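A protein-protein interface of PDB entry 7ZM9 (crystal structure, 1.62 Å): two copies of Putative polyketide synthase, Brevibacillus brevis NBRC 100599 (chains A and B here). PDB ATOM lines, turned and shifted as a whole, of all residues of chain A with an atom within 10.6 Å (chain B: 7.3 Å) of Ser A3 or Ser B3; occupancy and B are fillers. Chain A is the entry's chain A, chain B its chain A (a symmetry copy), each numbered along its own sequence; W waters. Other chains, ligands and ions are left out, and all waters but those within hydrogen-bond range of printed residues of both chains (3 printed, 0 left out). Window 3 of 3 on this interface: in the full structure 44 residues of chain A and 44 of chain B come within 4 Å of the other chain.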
ATOM      1  N   SER A   3     -10.457  23.623  14.709  1.00  0.00           N
ATOM      2  CA  SER A   3      -9.030  23.919  14.555  1.00  0.00           C
ATOM      3  C   SER A   3      -8.760  25.363  15.032  1.00  0.00           C
ATOM      4  O   SER A   3      -9.555  25.939  15.784  1.00  0.00           O
ATOM      5  CB  SER A   3      -8.577  23.708  13.100  1.00  0.00           C
ATOM      6  OG  SER A   3      -8.810  22.376  12.655  1.00  0.00           O
ATOM      7  N   VAL A   4      -7.648  25.946  14.593  1.00  0.00           N
ATOM      8  CA  VAL A   4      -7.164  27.198  15.167  1.00  0.00           C
ATOM      9  C   VAL A   4      -7.893  28.391  14.546  1.00  0.00           C
ATOM     10  O   VAL A   4      -8.399  28.337  13.422  1.00  0.00           O
ATOM     11  CB  VAL A   4      -5.630  27.305  14.988  1.00  0.00           C
ATOM     12  CG1 VAL A   4      -5.248  27.422  13.494  1.00  0.00           C
ATOM     13  CG2 VAL A   4      -5.066  28.476  15.814  1.00  0.00           C
ATOM     14  N   VAL A   5      -7.960  29.485  15.310  1.00  0.00           N
ATOM     15  CA  VAL A   5      -8.460  30.760  14.800  1.00  0.00           C
ATOM     16  C   VAL A   5      -7.632  31.197  13.603  1.00  0.00           C
ATOM     17  O   VAL A   5      -6.405  31.171  13.637  1.00  0.00           O
ATOM     18  CB  VAL A   5      -8.429  31.792  15.934  1.00  0.00           C
ATOM     19  CG1 VAL A   5      -8.902  33.141  15.459  1.00  0.00           C
ATOM     20  CG2 VAL A   5      -9.265  31.255  17.124  1.00  0.00           C
ATOM     21  N   ARG A   6      -8.296  31.545  12.516  1.00  0.00           N
ATOM     22  CA  ARG A   6      -7.603  32.066  11.357  1.00  0.00           C
ATOM     23  C   ARG A   6      -8.432  33.184  10.754  1.00  0.00           C
ATOM     24  O   ARG A   6      -9.610  33.361  11.064  1.00  0.00           O
ATOM     25  CB  ARG A   6      -7.302  31.029  10.295  1.00  0.00           C
ATOM     26  CG  ARG A   6      -8.444  30.189   9.845  1.00  0.00           C
ATOM     27  CD  ARG A   6      -7.867  28.906   9.253  1.00  0.00           C
ATOM     28  NE  ARG A   6      -8.793  28.134   8.430  1.00  0.00           N
ATOM     29  CZ  ARG A   6      -8.902  28.243   7.107  1.00  0.00           C
ATOM     30  NH1 ARG A   6      -8.162  29.118   6.429  1.00  0.00           N
ATOM     31  NH2 ARG A   6      -9.764  27.470   6.456  1.00  0.00           N
ATOM     32  N   ASP A   7      -7.805  33.974   9.885  1.00  0.00           N
ATOM     33  CA  ASP A   7      -8.495  35.152   9.387  1.00  0.00           C
ATOM     34  C   ASP A   7      -9.658  34.791   8.446  1.00  0.00           C
ATOM     35  O   ASP A   7      -9.547  33.906   7.586  1.00  0.00           O
ATOM     36  CB  ASP A   7      -7.529  36.068   8.624  1.00  0.00           C
ATOM     37  CG  ASP A   7      -6.527  36.770   9.518  1.00  0.00           C
ATOM     38  OD1 ASP A   7      -6.734  36.933  10.730  1.00  0.00           O
ATOM     39  OD2 ASP A   7      -5.492  37.163   8.959  1.00  0.00           O
ATOM     40  N   VAL A   8     -10.773  35.489   8.625  1.00  0.00           N
ATOM     41  CA  VAL A   8     -11.988  35.270   7.834  1.00  0.00           C
ATOM     42  C   VAL A   8     -12.367  36.544   7.111  1.00  0.00           C
ATOM     43  O   VAL A   8     -12.552  37.601   7.731  1.00  0.00           O
ATOM     44  CB  VAL A   8     -13.143  34.759   8.727  1.00  0.00           C
ATOM     45  CG1 VAL A   8     -14.458  34.769   7.963  1.00  0.00           C
ATOM     46  CG2 VAL A   8     -12.786  33.376   9.225  1.00  0.00           C
ATOM     47  N   HIS A 170     -20.132  34.710  15.893  1.00  0.00           N
ATOM     48  CA  HIS A 170     -19.140  33.931  16.601  1.00  0.00           C
ATOM     49  C   HIS A 170     -19.266  32.442  16.265  1.00  0.00           C
ATOM     50  O   HIS A 170     -18.251  31.764  16.037  1.00  0.00           O
ATOM     51  CB  HIS A 170     -19.270  34.142  18.110  1.00  0.00           C
ATOM     52  CG  HIS A 170     -18.327  33.320  18.915  1.00  0.00           C
ATOM     53  ND1 HIS A 170     -17.018  33.679  19.117  1.00  0.00           N
ATOM     54  CD2 HIS A 170     -18.483  32.126  19.538  1.00  0.00           C
ATOM     55  CE1 HIS A 170     -16.411  32.767  19.856  1.00  0.00           C
ATOM     56  NE2 HIS A 170     -17.277  31.778  20.080  1.00  0.00           N
ATOM     57  N   ALA A 172     -20.564  31.181  13.572  1.00  0.00           N
ATOM     58  CA  ALA A 172     -20.166  30.974  12.187  1.00  0.00           C
ATOM     59  C   ALA A 172     -18.648  30.875  12.053  1.00  0.00           C
ATOM     60  O   ALA A 172     -18.114  30.031  11.313  1.00  0.00           O
ATOM     61  CB  ALA A 172     -20.699  32.080  11.311  1.00  0.00           C
ATOM     62  N   LEU A 173     -17.929  31.749  12.752  1.00  0.00           N
ATOM     63  CA  LEU A 173     -16.473  31.724  12.742  1.00  0.00           C
ATOM     64  C   LEU A 173     -15.942  30.404  13.303  1.00  0.00           C
ATOM     65  O   LEU A 173     -15.044  29.784  12.723  1.00  0.00           O
ATOM     66  CB  LEU A 173     -15.928  32.892  13.565  1.00  0.00           C
ATOM     67  CG  LEU A 173     -16.252  34.270  13.018  1.00  0.00           C
ATOM     68  CD1 LEU A 173     -15.987  35.331  14.054  1.00  0.00           C
ATOM     69  CD2 LEU A 173     -15.431  34.528  11.788  1.00  0.00           C
ATOM     70  N   GLU A 174     -16.507  29.958  14.443  1.00  0.00           N
ATOM     71  CA  GLU A 174     -16.034  28.705  15.033  1.00  0.00           C
ATOM     72  C   GLU A 174     -16.282  27.542  14.076  1.00  0.00           C
ATOM     73  O   GLU A 174     -15.443  26.623  14.001  1.00  0.00           O
ATOM     74  CB  GLU A 174     -16.678  28.495  16.401  1.00  0.00           C
ATOM     75  CG  GLU A 174     -16.210  29.506  17.456  1.00  0.00           C
ATOM     76  CD  GLU A 174     -15.590  28.964  18.747  1.00  0.00           C
ATOM     77  OE1 GLU A 174     -14.516  29.490  19.115  1.00  0.00           O
ATOM     78  OE2 GLU A 174     -16.173  28.076  19.435  1.00  0.00           O
ATOM     79  N   SER A 175     -17.373  27.586  13.298  1.00  0.00           N
ATOM     80  CA  SER A 175     -17.667  26.561  12.292  1.00  0.00           C
ATOM     81  C   SER A 175     -16.674  26.621  11.132  1.00  0.00           C
ATOM     82  O   SER A 175     -16.170  25.591  10.663  1.00  0.00           O
ATOM     83  CB  SER A 175     -19.106  26.728  11.826  1.00  0.00           C
ATOM     84  OG  SER A 175     -19.402  25.912  10.711  1.00  0.00           O
ATOM     85  N   LEU A 176     -16.280  27.821  10.723  1.00  0.00           N
ATOM     86  CA  LEU A 176     -15.261  27.910   9.694  1.00  0.00           C
ATOM     87  C   LEU A 176     -13.917  27.423  10.217  1.00  0.00           C
ATOM     88  O   LEU A 176     -13.153  26.763   9.484  1.00  0.00           O
ATOM     89  CB  LEU A 176     -15.162  29.358   9.206  1.00  0.00           C
ATOM     90  CG  LEU A 176     -16.384  29.904   8.532  1.00  0.00           C
ATOM     91  CD1 LEU A 176     -16.338  31.398   8.413  1.00  0.00           C
ATOM     92  CD2 LEU A 176     -16.495  29.306   7.146  1.00  0.00           C
ATOM     93  N   TYR A 177     -13.604  27.711  11.481  1.00  0.00           N
ATOM     94  CA  TYR A 177     -12.302  27.275  11.998  1.00  0.00           C
ATOM     95  C   TYR A 177     -12.263  25.751  12.052  1.00  0.00           C
ATOM     96  O   TYR A 177     -11.237  25.120  11.774  1.00  0.00           O
ATOM     97  CB  TYR A 177     -12.055  27.798  13.402  1.00  0.00           C
ATOM     98  CG  TYR A 177     -12.089  29.296  13.582  1.00  0.00           C
ATOM     99  CD1 TYR A 177     -11.838  30.162  12.531  1.00  0.00           C
ATOM    100  CD2 TYR A 177     -12.405  29.832  14.812  1.00  0.00           C
ATOM    101  CE1 TYR A 177     -11.948  31.548  12.721  1.00  0.00           C
ATOM    102  CE2 TYR A 177     -12.473  31.239  15.002  1.00  0.00           C
ATOM    103  CZ  TYR A 177     -12.225  32.051  13.971  1.00  0.00           C
ATOM    104  OH  TYR A 177     -12.341  33.412  14.217  1.00  0.00           O
ATOM    105  N   SER A 178     -13.365  25.152  12.453  1.00  0.00           N
ATOM    106  CA  SER A 178     -13.335  23.689  12.603  1.00  0.00           C
ATOM    107  C   SER A 178     -13.592  22.954  11.308  1.00  0.00           C
ATOM    108  O   SER A 178     -13.418  21.714  11.262  1.00  0.00           O
ATOM    109  CB  SER A 178     -14.355  23.280  13.649  1.00  0.00           C
ATOM    110  OG  SER A 178     -15.587  23.480  13.136  1.00  0.00           O
ATOM    111  N   GLY A 179     -13.966  23.668  10.265  1.00  0.00           N
ATOM    112  CA  GLY A 179     -14.201  23.128   8.951  1.00  0.00           C
ATOM    113  C   GLY A 179     -15.557  22.497   8.748  1.00  0.00           C
ATOM    114  O   GLY A 179     -15.753  21.833   7.730  1.00  0.00           O
ATOM    115  N   THR A 180     -16.501  22.719   9.650  1.00  0.00           N
ATOM    116  CA  THR A 180     -17.863  22.243   9.411  1.00  0.00           C
ATOM    117  C   THR A 180     -18.626  23.096   8.412  1.00  0.00           C
ATOM    118  O   THR A 180     -19.629  22.630   7.860  1.00  0.00           O
ATOM    119  CB  THR A 180     -18.607  22.136  10.729  1.00  0.00           C
ATOM    120  OG1 THR A 180     -18.665  23.390  11.422  1.00  0.00           O
ATOM    121  CG2 THR A 180     -17.947  21.073  11.631  1.00  0.00           C
ATOM    122  N   SER A 181     -18.160  24.328   8.173  1.00  0.00           N
ATOM    123  CA  SER A 181     -18.595  25.208   7.104  1.00  0.00           C
ATOM    124  C   SER A 181     -17.341  25.548   6.289  1.00  0.00           C
ATOM    125  O   SER A 181     -16.247  25.684   6.856  1.00  0.00           O
ATOM    126  CB  SER A 181     -19.198  26.518   7.654  1.00  0.00           C
ATOM    127  OG  SER A 181     -20.409  26.358   8.411  1.00  0.00           O
ATOM    128  N   MET A 255     -15.279  36.631  20.593  1.00  0.00           N
ATOM    129  CA  MET A 255     -15.485  35.911  21.839  1.00  0.00           C
ATOM    130  C   MET A 255     -16.945  35.993  22.229  1.00  0.00           C
ATOM    131  O   MET A 255     -17.663  36.922  21.838  1.00  0.00           O
ATOM    132  CB  MET A 255     -14.588  36.489  22.915  1.00  0.00           C
ATOM    133  CG  MET A 255     -14.535  35.778  24.212  1.00  0.00           C
ATOM    134  SD  MET A 255     -14.040  34.049  24.043  1.00  0.00           S
ATOM    135  CE  MET A 255     -12.720  34.099  22.851  1.00  0.00           C
ATOM    136  N   ARG A 283      -7.433  36.443  21.198  1.00  0.00           N
ATOM    137  CA  ARG A 283      -7.686  35.527  20.098  1.00  0.00           C
ATOM    138  C   ARG A 283      -7.347  36.182  18.764  1.00  0.00           C
ATOM    139  O   ARG A 283      -6.840  35.522  17.864  1.00  0.00           O
ATOM    140  CB  ARG A 283      -9.146  35.060  20.115  1.00  0.00           C
ATOM    141  CG  ARG A 283      -9.488  34.417  18.819  1.00  0.00           C
ATOM    142  CD  ARG A 283     -10.940  33.863  18.849  1.00  0.00           C
ATOM    143  NE  ARG A 283     -10.974  32.754  19.804  1.00  0.00           N
ATOM    144  CZ  ARG A 283     -11.889  31.821  19.778  1.00  0.00           C
ATOM    145  NH1 ARG A 283     -12.822  31.925  18.876  1.00  0.00           N
ATOM    146  NH2 ARG A 283     -11.839  30.826  20.646  1.00  0.00           N
ATOM    147  N   SER B   3      -9.636  24.916  18.788  1.00  0.00           N
ATOM    148  CA  SER B   3      -8.516  23.983  18.633  1.00  0.00           C
ATOM    149  C   SER B   3      -9.065  22.609  18.189  1.00  0.00           C
ATOM    150  O   SER B   3     -10.183  22.512  17.671  1.00  0.00           O
ATOM    151  CB  SER B   3      -7.702  23.877  19.933  1.00  0.00           C
ATOM    152  OG  SER B   3      -7.182  25.136  20.342  1.00  0.00           O
ATOM    153  N   VAL B   4      -8.284  21.552  18.397  1.00  0.00           N
ATOM    154  CA  VAL B   4      -8.582  20.253  17.801  1.00  0.00           C
ATOM    155  C   VAL B   4      -9.620  19.502  18.637  1.00  0.00           C
ATOM    156  O   VAL B   4      -9.773  19.722  19.842  1.00  0.00           O
ATOM    157  CB  VAL B   4      -7.278  19.436  17.634  1.00  0.00           C
ATOM    158  CG1 VAL B   4      -6.667  19.069  19.007  1.00  0.00           C
ATOM    159  CG2 VAL B   4      -7.526  18.185  16.769  1.00  0.00           C
ATOM    160  N   VAL B   5     -10.358  18.610  17.971  1.00  0.00           N
ATOM    161  CA  VAL B   5     -11.263  17.687  18.653  1.00  0.00           C
ATOM    162  C   VAL B   5     -10.486  16.848  19.654  1.00  0.00           C
ATOM    163  O   VAL B   5      -9.432  16.302  19.342  1.00  0.00           O
ATOM    164  CB  VAL B   5     -11.973  16.824  17.602  1.00  0.00           C
ATOM    165  CG1 VAL B   5     -12.896  15.826  18.247  1.00  0.00           C
ATOM    166  CG2 VAL B   5     -12.708  17.756  16.603  1.00  0.00           C
ATOM    167  N   ARG B   6     -10.971  16.787  20.881  1.00  0.00           N
ATOM    168  CA  ARG B   6     -10.357  15.939  21.880  1.00  0.00           C
ATOM    169  C   ARG B   6     -11.451  15.302  22.718  1.00  0.00           C
ATOM    170  O   ARG B   6     -12.612  15.711  22.693  1.00  0.00           O
ATOM    171  CB  ARG B   6      -9.377  16.656  22.787  1.00  0.00           C
ATOM    172  CG  ARG B   6      -9.863  17.903  23.435  1.00  0.00           C
ATOM    173  CD  ARG B   6      -8.639  18.735  23.807  1.00  0.00           C
ATOM    174  NE  ARG B   6      -8.886  19.801  24.773  1.00  0.00           N
ATOM    175  CZ  ARG B   6      -8.731  19.681  26.091  1.00  0.00           C
ATOM    176  NH1 ARG B   6      -8.351  18.525  26.632  1.00  0.00           N
ATOM    177  NH2 ARG B   6      -8.963  20.727  26.875  1.00  0.00           N
ATOM    178  N   GLU B 174     -17.699  22.115  20.775  1.00  0.00           N
ATOM    179  CA  GLU B 174     -16.845  23.035  20.023  1.00  0.00           C
ATOM    180  C   GLU B 174     -16.300  24.124  20.944  1.00  0.00           C
ATOM    181  O   GLU B 174     -15.139  24.542  20.775  1.00  0.00           O
ATOM    182  CB  GLU B 174     -17.609  23.597  18.827  1.00  0.00           C
ATOM    183  CG  GLU B 174     -17.916  22.546  17.753  1.00  0.00           C
ATOM    184  CD  GLU B 174     -17.426  22.810  16.326  1.00  0.00           C
ATOM    185  OE1 GLU B 174     -16.834  21.867  15.755  1.00  0.00           O
ATOM    186  OE2 GLU B 174     -17.667  23.905  15.739  1.00  0.00           O
ATOM    187  N   SER B 175     -17.080  24.548  21.950  1.00  0.00           N
ATOM    188  CA  SER B 175     -16.627  25.533  22.936  1.00  0.00           C
ATOM    189  C   SER B 175     -15.542  24.953  23.843  1.00  0.00           C
ATOM    190  O   SER B 175     -14.526  25.603  24.127  1.00  0.00           O
ATOM    191  CB  SER B 175     -17.831  26.028  23.724  1.00  0.00           C
ATOM    192  OG  SER B 175     -17.453  26.824  24.830  1.00  0.00           O
ATOM    193  N   LEU B 176     -15.670  23.687  24.220  1.00  0.00           N
ATOM    194  CA  LEU B 176     -14.606  23.076  24.995  1.00  0.00           C
ATOM    195  C   LEU B 176     -13.347  22.911  24.155  1.00  0.00           C
ATOM    196  O   LEU B 176     -12.221  23.098  24.657  1.00  0.00           O
ATOM    197  CB  LEU B 176     -15.083  21.723  25.529  1.00  0.00           C
ATOM    198  CG  LEU B 176     -16.231  21.770  26.492  1.00  0.00           C
ATOM    199  CD1 LEU B 176     -16.859  20.421  26.682  1.00  0.00           C
ATOM    200  CD2 LEU B 176     -15.735  22.272  27.831  1.00  0.00           C
ATOM    201  N   TYR B 177     -13.499  22.583  22.871  1.00  0.00           N
ATOM    202  CA  TYR B 177     -12.299  22.393  22.049  1.00  0.00           C
ATOM    203  C   TYR B 177     -11.570  23.724  21.902  1.00  0.00           C
ATOM    204  O   TYR B 177     -10.335  23.790  21.905  1.00  0.00           O
ATOM    205  CB  TYR B 177     -12.648  21.896  20.658  1.00  0.00           C
ATOM    206  CG  TYR B 177     -13.414  20.598  20.575  1.00  0.00           C
ATOM    207  CD1 TYR B 177     -13.363  19.656  21.589  1.00  0.00           C
ATOM    208  CD2 TYR B 177     -14.212  20.340  19.481  1.00  0.00           C
ATOM    209  CE1 TYR B 177     -14.145  18.493  21.508  1.00  0.00           C
ATOM    210  CE2 TYR B 177     -14.967  19.139  19.391  1.00  0.00           C
ATOM    211  CZ  TYR B 177     -14.899  18.249  20.384  1.00  0.00           C
ATOM    212  OH  TYR B 177     -15.686  17.114  20.248  1.00  0.00           O
ATOM    213  N   SER B 178     -12.325  24.788  21.727  1.00  0.00           N
ATOM    214  CA  SER B 178     -11.654  26.075  21.492  1.00  0.00           C
ATOM    215  C   SER B 178     -11.239  26.771  22.767  1.00  0.00           C
ATOM    216  O   SER B 178     -10.504  27.783  22.702  1.00  0.00           O
ATOM    217  CB  SER B 178     -12.574  26.971  20.682  1.00  0.00           C
ATOM    218  OG  SER B 178     -13.606  27.337  21.471  1.00  0.00           O
ATOM    219  N   GLY B 179     -11.655  26.255  23.907  1.00  0.00           N
ATOM    220  CA  GLY B 179     -11.308  26.767  25.207  1.00  0.00           C
ATOM    221  C   GLY B 179     -12.131  27.943  25.675  1.00  0.00           C
ATOM    222  O   GLY B 179     -11.759  28.564  26.673  1.00  0.00           O
ATOM    223  N   ARG B 283     -14.472  12.550  12.520  1.00  0.00           N
ATOM    224  CA  ARG B 283     -14.014  13.414  13.595  1.00  0.00           C
ATOM    225  C   ARG B 283     -13.727  12.603  14.853  1.00  0.00           C
ATOM    226  O   ARG B 283     -12.783  12.899  15.577  1.00  0.00           O
ATOM    227  CB  ARG B 283     -15.051  14.506  13.883  1.00  0.00           C
ATOM    228  CG  ARG B 283     -14.752  15.160  15.184  1.00  0.00           C
ATOM    229  CD  ARG B 283     -15.744  16.326  15.452  1.00  0.00           C
ATOM    230  NE  ARG B 283     -15.474  17.376  14.469  1.00  0.00           N
ATOM    231  CZ  ARG B 283     -15.818  18.625  14.648  1.00  0.00           C
ATOM    232  NH1 ARG B 283     -16.461  18.915  15.742  1.00  0.00           N
ATOM    233  NH2 ARG B 283     -15.509  19.529  13.736  1.00  0.00           N
HETATM  234  O   HOH W   1     -10.224  30.340  23.174  1.00  0.00           O
HETATM  235  O   HOH W   2     -19.549  23.297  13.938  1.00  0.00           O
HETATM  236  O   HOH W   3     -14.472  19.352  10.885  1.00  0.00           O
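Water W3 bridges the backbone carbonyl oxygen of Ser A178 (2.6 Å) and the guanidinium group of Arg B283 (3.0 Å). Water W1 bridges O of Ser B178 (2.6 Å) and NH2 of Arg A283 (3.0 Å). Water W2 bridges OG1 of Thr A180 and OE2 of Glu B174.
The backbone NH (N) of Ser A3 sits close to the backbone carbonyl oxygen (O) of Tyr A177 (3.4 Å). The side-chain hydroxyl (OG) of Ser A178 lies within hydrogen-bond range of the backbone carbonyl oxygen (O) of Glu A174, at 3.3 Å. NH1 of Arg A283 is in salt-bridge range of OE1 of Glu A174 (3.0 Å). The backbone carbonyl oxygen (O) of Ser A175 is in hydrogen-bond range of the side-chain hydroxyl (OG) of Ser A178. The backbone carbonyl oxygen (O) of Tyr B177 sits close to the backbone NH (N) of Ser B3 (3.4 Å). The backbone carbonyl oxygen of Glu B174 lies within hydrogen-bond range of the side-chain hydroxyl of Ser B178 (3.3 Å).
The backbone NH (N) of Ser A3 lies within hydrogen-bond range of the backbone carbonyl oxygen (O) of Ser B3. The side-chain hydroxyl (OG) of Ser B178 is in hydrogen-bond range of the side-chain carboxylate (OE1) of Glu A174 (3.3 Å). OG of Ser A178 lies within hydrogen-bond range of OE1 of Glu B174.
Ser A3 touches one residue of chain B. Printed residues of chain B within 4 Å of Glu A174: Glu B174 (3.9 Å) and Ser B178 (3.3 Å). Ser B3 touches just one residue of chain A: Ser A3. Val B4 touches none of the printed residues of chain A. Of the printed residues of chain A, Ser B178 touches Glu A174 (3.3 Å) and Arg A283 (3.9 Å). Of the printed residues of chain A, Arg B283 touches Ser A178 and Thr A180. The nearest residue of chain B that does not touch Ser A3 is Val B4 (4.6 Å).
Of the 19 printed residues of chain A, 5 touch a printed residue of chain B. Printed residues of chain A that touch a printed residue of chain B: Ser A3, Glu A174, Ser A178, Thr A180 and Arg A283. Printed residues of chain B that touch a printed residue of chain A: Ser B3, Glu B174, Ser B178 and Arg B283. Among the printed residues, 7 pairs touch across the chains. Among the printed residues, no Asp or Glu carboxylate lies within 4 Å of a Lys or Arg side-chain nitrogen of the other chain.
Among the printed residues, pairs that only touch across the chains: Thr A180 with Arg B283, Ser A178 with Arg B283, Arg A283 with Ser B178 and Glu A174 with Glu B174.
Ser B3 touches its own counterpart, Ser A3. Glu B174 touches its own counterpart, Glu A174. Glu A174 touches Ser B178, and with the chains exchanged Ser A178 touches Glu B174. Ser A178 touches Arg B283, and with the chains exchanged Arg A283 touches Ser B178. 11 positions are printed for both chains.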
